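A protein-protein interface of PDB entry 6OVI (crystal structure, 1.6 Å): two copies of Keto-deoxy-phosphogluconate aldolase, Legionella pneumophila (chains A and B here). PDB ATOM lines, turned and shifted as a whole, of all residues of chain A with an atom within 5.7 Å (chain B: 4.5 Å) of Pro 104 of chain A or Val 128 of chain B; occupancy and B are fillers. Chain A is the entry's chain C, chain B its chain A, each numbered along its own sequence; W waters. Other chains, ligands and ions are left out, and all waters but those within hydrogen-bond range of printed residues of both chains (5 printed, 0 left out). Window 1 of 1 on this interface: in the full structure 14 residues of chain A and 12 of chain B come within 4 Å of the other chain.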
ATOM      1  N   THR A  83      30.855  -5.562  28.748  1.00  0.00           N
ATOM      2  CA  THR A  83      31.064  -4.638  27.625  1.00  0.00           C
ATOM      3  C   THR A  83      30.231  -5.062  26.413  1.00  0.00           C
ATOM      4  O   THR A  83      30.651  -4.972  25.256  1.00  0.00           O
ATOM      5  CB  THR A  83      32.547  -4.527  27.266  1.00  0.00           C
ATOM      6  OG1 THR A  83      33.327  -4.557  28.470  1.00  0.00           O
ATOM      7  CG2 THR A  83      32.816  -3.207  26.535  1.00  0.00           C
ATOM      8  N   VAL A  84      29.029  -5.552  26.689  1.00  0.00           N
ATOM      9  CA  VAL A  84      28.095  -5.907  25.629  1.00  0.00           C
ATOM     10  C   VAL A  84      27.376  -4.630  25.212  1.00  0.00           C
ATOM     11  O   VAL A  84      26.543  -4.108  25.957  1.00  0.00           O
ATOM     12  CB  VAL A  84      27.112  -6.982  26.095  1.00  0.00           C
ATOM     13  CG1 VAL A  84      26.093  -7.301  24.991  1.00  0.00           C
ATOM     14  CG2 VAL A  84      27.891  -8.228  26.550  1.00  0.00           C
ATOM     15  N   ILE A  85      27.726  -4.101  24.044  1.00  0.00           N
ATOM     16  CA  ILE A  85      27.226  -2.804  23.588  1.00  0.00           C
ATOM     17  C   ILE A  85      26.029  -2.951  22.649  1.00  0.00           C
ATOM     18  O   ILE A  85      25.034  -2.234  22.780  1.00  0.00           O
ATOM     19  CB  ILE A  85      28.362  -1.997  22.917  1.00  0.00           C
ATOM     20  CG1 ILE A  85      29.568  -1.885  23.841  1.00  0.00           C
ATOM     21  CG2 ILE A  85      27.853  -0.612  22.492  1.00  0.00           C
ATOM     22  CD1 ILE A  85      29.228  -1.477  25.236  1.00  0.00           C
ATOM     23  N   ILE A 102      26.371  -8.074  30.695  1.00  0.00           N
ATOM     24  CA  ILE A 102      26.451  -6.776  31.357  1.00  0.00           C
ATOM     25  C   ILE A 102      26.860  -5.728  30.330  1.00  0.00           C
ATOM     26  O   ILE A 102      27.716  -5.987  29.476  1.00  0.00           O
ATOM     27  CB  ILE A 102      27.453  -6.831  32.528  1.00  0.00           C
ATOM     28  CG1 ILE A 102      26.971  -7.866  33.553  1.00  0.00           C
ATOM     29  CG2 ILE A 102      27.632  -5.442  33.131  1.00  0.00           C
ATOM     30  CD1 ILE A 102      27.921  -8.035  34.711  1.00  0.00           C
ATOM     31  N   SER A 103      26.240  -4.551  30.403  1.00  0.00           N
ATOM     32  CA  SER A 103      26.589  -3.452  29.511  1.00  0.00           C
ATOM     33  C   SER A 103      26.963  -2.215  30.315  1.00  0.00           C
ATOM     34  O   SER A 103      26.434  -2.004  31.408  1.00  0.00           O
ATOM     35  CB  SER A 103      25.399  -3.123  28.594  1.00  0.00           C
ATOM     36  OG  SER A 103      25.736  -2.127  27.645  1.00  0.00           O
ATOM     37  N   PRO A 104      27.856  -1.361  29.795  1.00  0.00           N
ATOM     38  CA  PRO A 104      28.170  -0.108  30.497  1.00  0.00           C
ATOM     39  C   PRO A 104      27.107   0.966  30.355  1.00  0.00           C
ATOM     40  O   PRO A 104      27.181   1.974  31.071  1.00  0.00           O
ATOM     41  CB  PRO A 104      29.479   0.348  29.834  1.00  0.00           C
ATOM     42  CG  PRO A 104      29.423  -0.213  28.493  1.00  0.00           C
ATOM     43  CD  PRO A 104      28.743  -1.572  28.641  1.00  0.00           C
ATOM     44  N   GLY A 105      26.145   0.769  29.474  1.00  0.00           N
ATOM     45  CA  GLY A 105      25.071   1.722  29.263  1.00  0.00           C
ATOM     46  C   GLY A 105      23.891   0.985  28.673  1.00  0.00           C
ATOM     47  O   GLY A 105      23.737  -0.226  28.869  1.00  0.00           O
ATOM     48  N   GLN A 106      23.037   1.711  27.954  1.00  0.00           N
ATOM     49  CA  GLN A 106      21.865   1.089  27.361  1.00  0.00           C
ATOM     50  C   GLN A 106      21.388   1.903  26.167  1.00  0.00           C
ATOM     51  O   GLN A 106      21.652   3.107  26.060  1.00  0.00           O
ATOM     52  CB  GLN A 106      20.746   0.938  28.399  1.00  0.00           C
ATOM     53  CG  GLN A 106      20.377   2.229  29.088  1.00  0.00           C
ATOM     54  CD  GLN A 106      19.058   2.773  28.596  1.00  0.00           C
ATOM     55  OE1 GLN A 106      18.758   2.714  27.403  1.00  0.00           O
ATOM     56  NE2 GLN A 106      18.247   3.274  29.510  1.00  0.00           N
ATOM     57  N   PRO A 123      21.860  -3.863  32.251  1.00  0.00           N
ATOM     58  CA  PRO A 123      22.288  -2.662  31.531  1.00  0.00           C
ATOM     59  C   PRO A 123      22.891  -1.632  32.466  1.00  0.00           C
ATOM     60  O   PRO A 123      22.683  -1.646  33.676  1.00  0.00           O
ATOM     61  CB  PRO A 123      20.982  -2.134  30.915  1.00  0.00           C
ATOM     62  CG  PRO A 123      19.890  -2.662  31.796  1.00  0.00           C
ATOM     63  CD  PRO A 123      20.413  -3.885  32.524  1.00  0.00           C
ATOM     64  N   GLY A 124      23.641  -0.713  31.866  1.00  0.00           N
ATOM     65  CA  GLY A 124      24.248   0.372  32.613  1.00  0.00           C
ATOM     66  C   GLY A 124      23.400   1.627  32.544  1.00  0.00           C
ATOM     67  O   GLY A 124      22.773   1.914  31.528  1.00  0.00           O
ATOM     68  N   VAL A 125      23.374   2.373  33.653  1.00  0.00           N
ATOM     69  CA  VAL A 125      22.763   3.696  33.669  1.00  0.00           C
ATOM     70  C   VAL A 125      23.639   4.642  34.478  1.00  0.00           C
ATOM     71  O   VAL A 125      24.453   4.226  35.308  1.00  0.00           O
ATOM     72  CB  VAL A 125      21.322   3.694  34.235  1.00  0.00           C
ATOM     73  CG1 VAL A 125      20.393   2.815  33.391  1.00  0.00           C
ATOM     74  CG2 VAL A 125      21.319   3.241  35.671  1.00  0.00           C
ATOM     75  N   ALA A 126      23.479   5.937  34.205  1.00  0.00           N
ATOM     76  CA  ALA A 126      24.182   6.961  34.978  1.00  0.00           C
ATOM     77  C   ALA A 126      23.301   8.133  35.379  1.00  0.00           C
ATOM     78  O   ALA A 126      23.734   8.943  36.199  1.00  0.00           O
ATOM     79  CB  ALA A 126      25.383   7.504  34.203  1.00  0.00           C
ATOM     80  N   GLU A 130      17.861   7.757  32.428  1.00  0.00           N
ATOM     81  CA  GLU A 130      18.281   6.456  31.916  1.00  0.00           C
ATOM     82  C   GLU A 130      17.700   5.325  32.755  1.00  0.00           C
ATOM     83  O   GLU A 130      17.189   4.336  32.211  1.00  0.00           O
ATOM     84  CB  GLU A 130      19.811   6.402  31.878  1.00  0.00           C
ATOM     85  CG  GLU A 130      20.341   7.353  30.807  1.00  0.00           C
ATOM     86  CD  GLU A 130      21.828   7.657  30.905  1.00  0.00           C
ATOM     87  OE1 GLU A 130      22.522   7.087  31.786  1.00  0.00           O
ATOM     88  OE2 GLU A 130      22.297   8.493  30.083  1.00  0.00           O
ATOM     89  N   LYS A 143      23.935  -1.830  36.213  1.00  0.00           N
ATOM     90  CA  LYS A 143      25.268  -1.323  36.449  1.00  0.00           C
ATOM     91  C   LYS A 143      25.188   0.199  36.552  1.00  0.00           C
ATOM     92  O   LYS A 143      24.470   0.840  35.777  1.00  0.00           O
ATOM     93  CB  LYS A 143      26.164  -1.762  35.297  1.00  0.00           C
ATOM     94  CG  LYS A 143      27.602  -1.355  35.363  1.00  0.00           C
ATOM     95  CD  LYS A 143      28.332  -2.134  34.274  1.00  0.00           C
ATOM     96  CE  LYS A 143      29.724  -1.635  34.004  1.00  0.00           C
ATOM     97  NZ  LYS A 143      30.120  -2.083  32.640  1.00  0.00           N
ATOM     98  N   PHE A 145      27.561   3.190  36.057  1.00  0.00           N
ATOM     99  CA  PHE A 145      28.837   3.323  35.416  1.00  0.00           C
ATOM    100  C   PHE A 145      29.002   4.637  34.673  1.00  0.00           C
ATOM    101  O   PHE A 145      28.106   5.047  33.924  1.00  0.00           O
ATOM    102  CB  PHE A 145      29.049   2.175  34.421  1.00  0.00           C
ATOM    103  CG  PHE A 145      30.361   2.267  33.686  1.00  0.00           C
ATOM    104  CD1 PHE A 145      31.521   1.785  34.267  1.00  0.00           C
ATOM    105  CD2 PHE A 145      30.445   2.858  32.440  1.00  0.00           C
ATOM    106  CE1 PHE A 145      32.723   1.878  33.616  1.00  0.00           C
ATOM    107  CE2 PHE A 145      31.656   2.958  31.775  1.00  0.00           C
ATOM    108  CZ  PHE A 145      32.805   2.467  32.367  1.00  0.00           C
ATOM    109  N   PRO A 146      30.153   5.295  34.809  1.00  0.00           N
ATOM    110  CA  PRO A 146      31.254   4.959  35.720  1.00  0.00           C
ATOM    111  C   PRO A 146      30.989   5.589  37.078  1.00  0.00           C
ATOM    112  O   PRO A 146      30.907   6.808  37.180  1.00  0.00           O
ATOM    113  CB  PRO A 146      32.481   5.559  35.032  1.00  0.00           C
ATOM    114  CG  PRO A 146      31.946   6.658  34.198  1.00  0.00           C
ATOM    115  CD  PRO A 146      30.508   6.361  33.867  1.00  0.00           C
ATOM    116  N   SER B 127      27.164  10.832  28.745  1.00  0.00           N
ATOM    117  CA  SER B 127      26.998   9.570  29.449  1.00  0.00           C
ATOM    118  C   SER B 127      27.253   8.460  28.454  1.00  0.00           C
ATOM    119  O   SER B 127      27.223   8.679  27.239  1.00  0.00           O
ATOM    120  CB  SER B 127      25.597   9.391  30.050  1.00  0.00           C
ATOM    121  OG  SER B 127      24.657   9.088  29.026  1.00  0.00           O
ATOM    122  N   VAL B 128      27.508   7.266  28.988  1.00  0.00           N
ATOM    123  CA  VAL B 128      27.778   6.118  28.129  1.00  0.00           C
ATOM    124  C   VAL B 128      26.542   5.749  27.320  1.00  0.00           C
ATOM    125  O   VAL B 128      26.648   5.337  26.159  1.00  0.00           O
ATOM    126  CB  VAL B 128      28.295   4.936  28.968  1.00  0.00           C
ATOM    127  CG1 VAL B 128      28.274   3.638  28.143  1.00  0.00           C
ATOM    128  CG2 VAL B 128      29.692   5.245  29.438  1.00  0.00           C
ATOM    129  N   SER B 129      25.355   5.890  27.906  1.00  0.00           N
ATOM    130  CA  SER B 129      24.148   5.581  27.142  1.00  0.00           C
ATOM    131  C   SER B 129      23.972   6.554  25.980  1.00  0.00           C
ATOM    132  O   SER B 129      23.535   6.159  24.893  1.00  0.00           O
ATOM    133  CB  SER B 129      22.904   5.586  28.039  1.00  0.00           C
ATOM    134  OG  SER B 129      22.941   4.514  28.982  1.00  0.00           O
ATOM    135  N   GLU B 130      24.272   7.832  26.199  1.00  0.00           N
ATOM    136  CA  GLU B 130      24.189   8.793  25.105  1.00  0.00           C
ATOM    137  C   GLU B 130      25.204   8.455  24.019  1.00  0.00           C
ATOM    138  O   GLU B 130      24.879   8.467  22.823  1.00  0.00           O
ATOM    139  CB  GLU B 130      24.387  10.214  25.650  1.00  0.00           C
ATOM    140  CG  GLU B 130      23.178  10.638  26.488  1.00  0.00           C
ATOM    141  CD  GLU B 130      23.402  11.906  27.302  1.00  0.00           C
ATOM    142  OE1 GLU B 130      24.454  12.548  27.144  1.00  0.00           O
ATOM    143  OE2 GLU B 130      22.506  12.257  28.118  1.00  0.00           O
ATOM    144  N   LEU B 131      26.427   8.121  24.420  1.00  0.00           N
ATOM    145  CA  LEU B 131      27.425   7.649  23.463  1.00  0.00           C
ATOM    146  C   LEU B 131      26.894   6.467  22.662  1.00  0.00           C
ATOM    147  O   LEU B 131      27.006   6.429  21.427  1.00  0.00           O
ATOM    148  CB  LEU B 131      28.701   7.271  24.215  1.00  0.00           C
ATOM    149  CG  LEU B 131      29.952   6.832  23.464  1.00  0.00           C
ATOM    150  CD1 LEU B 131      31.128   6.984  24.402  1.00  0.00           C
ATOM    151  CD2 LEU B 131      29.863   5.389  23.006  1.00  0.00           C
ATOM    152  N   MET B 132      26.299   5.487  23.353  1.00  0.00           N
ATOM    153  CA  MET B 132      25.843   4.279  22.675  1.00  0.00           C
ATOM    154  C   MET B 132      24.712   4.582  21.707  1.00  0.00           C
ATOM    155  O   MET B 132      24.618   3.949  20.654  1.00  0.00           O
ATOM    156  CB  MET B 132      25.421   3.214  23.692  1.00  0.00           C
ATOM    157  CG  MET B 132      26.641   2.617  24.404  1.00  0.00           C
ATOM    158  SD  MET B 132      26.220   1.529  25.774  1.00  0.00           S
ATOM    159  CE  MET B 132      25.055   0.376  25.016  1.00  0.00           C
ATOM    160  N   ILE B 159      35.641   5.944  30.171  1.00  0.00           N
ATOM    161  CA  ILE B 159      35.031   5.626  28.884  1.00  0.00           C
ATOM    162  C   ILE B 159      36.070   5.081  27.920  1.00  0.00           C
ATOM    163  O   ILE B 159      35.764   4.210  27.098  1.00  0.00           O
ATOM    164  CB  ILE B 159      34.319   6.881  28.337  1.00  0.00           C
ATOM    165  CG1 ILE B 159      33.135   7.232  29.251  1.00  0.00           C
ATOM    166  CG2 ILE B 159      33.864   6.693  26.890  1.00  0.00           C
ATOM    167  CD1 ILE B 159      32.451   8.537  28.896  1.00  0.00           C
ATOM    168  N   PHE B 163      35.338   2.054  25.262  1.00  0.00           N
ATOM    169  CA  PHE B 163      35.137   2.486  23.876  1.00  0.00           C
ATOM    170  C   PHE B 163      36.423   3.091  23.326  1.00  0.00           C
ATOM    171  O   PHE B 163      36.488   4.298  23.052  1.00  0.00           O
ATOM    172  CB  PHE B 163      33.994   3.497  23.776  1.00  0.00           C
ATOM    173  CG  PHE B 163      32.675   2.977  24.269  1.00  0.00           C
ATOM    174  CD1 PHE B 163      31.824   2.289  23.424  1.00  0.00           C
ATOM    175  CD2 PHE B 163      32.282   3.191  25.584  1.00  0.00           C
ATOM    176  CE1 PHE B 163      30.601   1.818  23.879  1.00  0.00           C
ATOM    177  CE2 PHE B 163      31.065   2.727  26.042  1.00  0.00           C
ATOM    178  CZ  PHE B 163      30.224   2.040  25.188  1.00  0.00           C
HETATM  179  O   HOH W   1      27.848   7.254  31.845  1.00  0.00           O
HETATM  180  O   HOH W   2      22.602  11.297  30.748  1.00  0.00           O
HETATM  181  O   HOH W   3      24.683   5.845  30.727  1.00  0.00           O
HETATM  182  O   HOH W   4      20.772  10.356  29.020  1.00  0.00           O
HETATM  183  O   HOH W   5      20.429   5.346  24.949  1.00  0.00           O
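OE2 of Glu 130 of chain A is in hydrogen-bond range of OG of Ser 127 of chain B (2.7 Å). OG of Ser 129 of chain B lies within hydrogen-bond range of N of Gln 106 of chain A. The side-chain sulfur of Met 132 of chain B lies close to the backbone NH of Gly 105 of chain A (3.8 Å).
The side-chain hydroxyl (OG) of Ser 127 of chain B lies close to the backbone NH (N) of Ser 129 of chain B (3.5 Å). N of Glu 130 of chain B sits at hydrogen-bond distance from OG of Ser 127 of chain B, 3.1 Å away. OG of Ser 103 of chain A is in hydrogen-bond range of O of Gly 105 of chain A, 3.0 Å away. The backbone carbonyl oxygen (O) of Ser 103 of chain A sits at hydrogen-bond distance from the backbone NH (N) of Gly 124 of chain A. O of Glu 130 of chain A sits at hydrogen-bond distance from NE2 of Gln 106 of chain A, 3.1 Å away. The backbone NH (N) of Phe 145 of chain A is in hydrogen-bond range of the backbone carbonyl oxygen (O) of Val 125 of chain A, at 3.4 Å.
Among the printed residues, pairs that only touch across the chains: Ile 85 of chain A with Met 132 of chain B (3.4 Å), Gly 105 of chain A with Ser 129 of chain B (3.5 Å), Pro 104 of chain A with Val 128 of chain B (3.5 Å), Glu 130 of chain A with Ser 129 of chain B (3.6 Å), Gly 124 of chain A with Ser 129 of chain B (3.6 Å), Ile 85 of chain A with Phe 163 of chain B (3.7 Å), Ser 103 of chain A with Met 132 of chain B (3.7 Å), Gln 106 of chain A with Met 132 of chain B (3.8 Å), Gly 105 of chain A with Val 128 of chain B (3.8 Å) and Phe 145 of chain A with Val 128 of chain B (3.8 Å).
Val 128 of chain B touches just these residues of chain A: Pro 104, Gly 105 and Phe 145. Of the printed residues of chain B, Gly 105 of chain A touches Val 128, Ser 129 and Met 132. Printed residues of chain B within 4 Å of Gly 124 of chain A: Ser 129 (3.6 Å). Of the printed residues of chain B, Ile 85 of chain A touches Met 132 and Phe 163. Lys 143 of chain A touches none of the printed residues of chain B. Pro 123 of chain A touches none of the printed residues of chain B. The nearest printed residue of chain B that does not touch Pro 104 of chain A is Phe 163 of chain B (4.1 Å).
Printed residues of chain B that touch a printed residue of chain A: Ser 127, Val 128, Ser 129, Met 132 and Phe 163. Hydrophobic or aromatic side chains of chain B that line the printed part of chain A: Val 128, Met 132 and Phe 163. Printed residues of chain A that touch a printed residue of chain B: Ile 85, Ser 103, Pro 104, Gly 105, Gln 106, Gly 124, Glu 130 and Phe 145.
1 position is printed for both chains. Of the 13 pairs that touch across the chains among the printed residues, none has its exchanged pair printed and touching as well.
Water W4 bridges the side-chain carboxylate of Glu 130 of chain A and the side-chain carboxylate of Glu 130 of chain B. Water W3 lies within hydrogen-bond range of OE1 of Glu 130 of chain A (2.7 Å) and OG of Ser 129 of chain B (2.8 Å). Water W5 lies within hydrogen-bond range of the backbone carbonyl oxygen of Gln 106 of chain A (2.8 Å) and the backbone carbonyl oxygen of Ser 129 of chain B (3.2 Å). Water W2 lies within hydrogen-bond range of the side-chain carboxylate (OE2) of Glu 130 of chain B (2.8 Å), the side-chain carboxylate (OE2) of Glu 130 of chain A (2.9 Å) and the side-chain hydroxyl (OG) of Ser 127 of chain B (3.5 Å). Water W1 bridges the backbone NH of Val 128 of chain B and the backbone carbonyl oxygen of Phe 145 of chain A.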
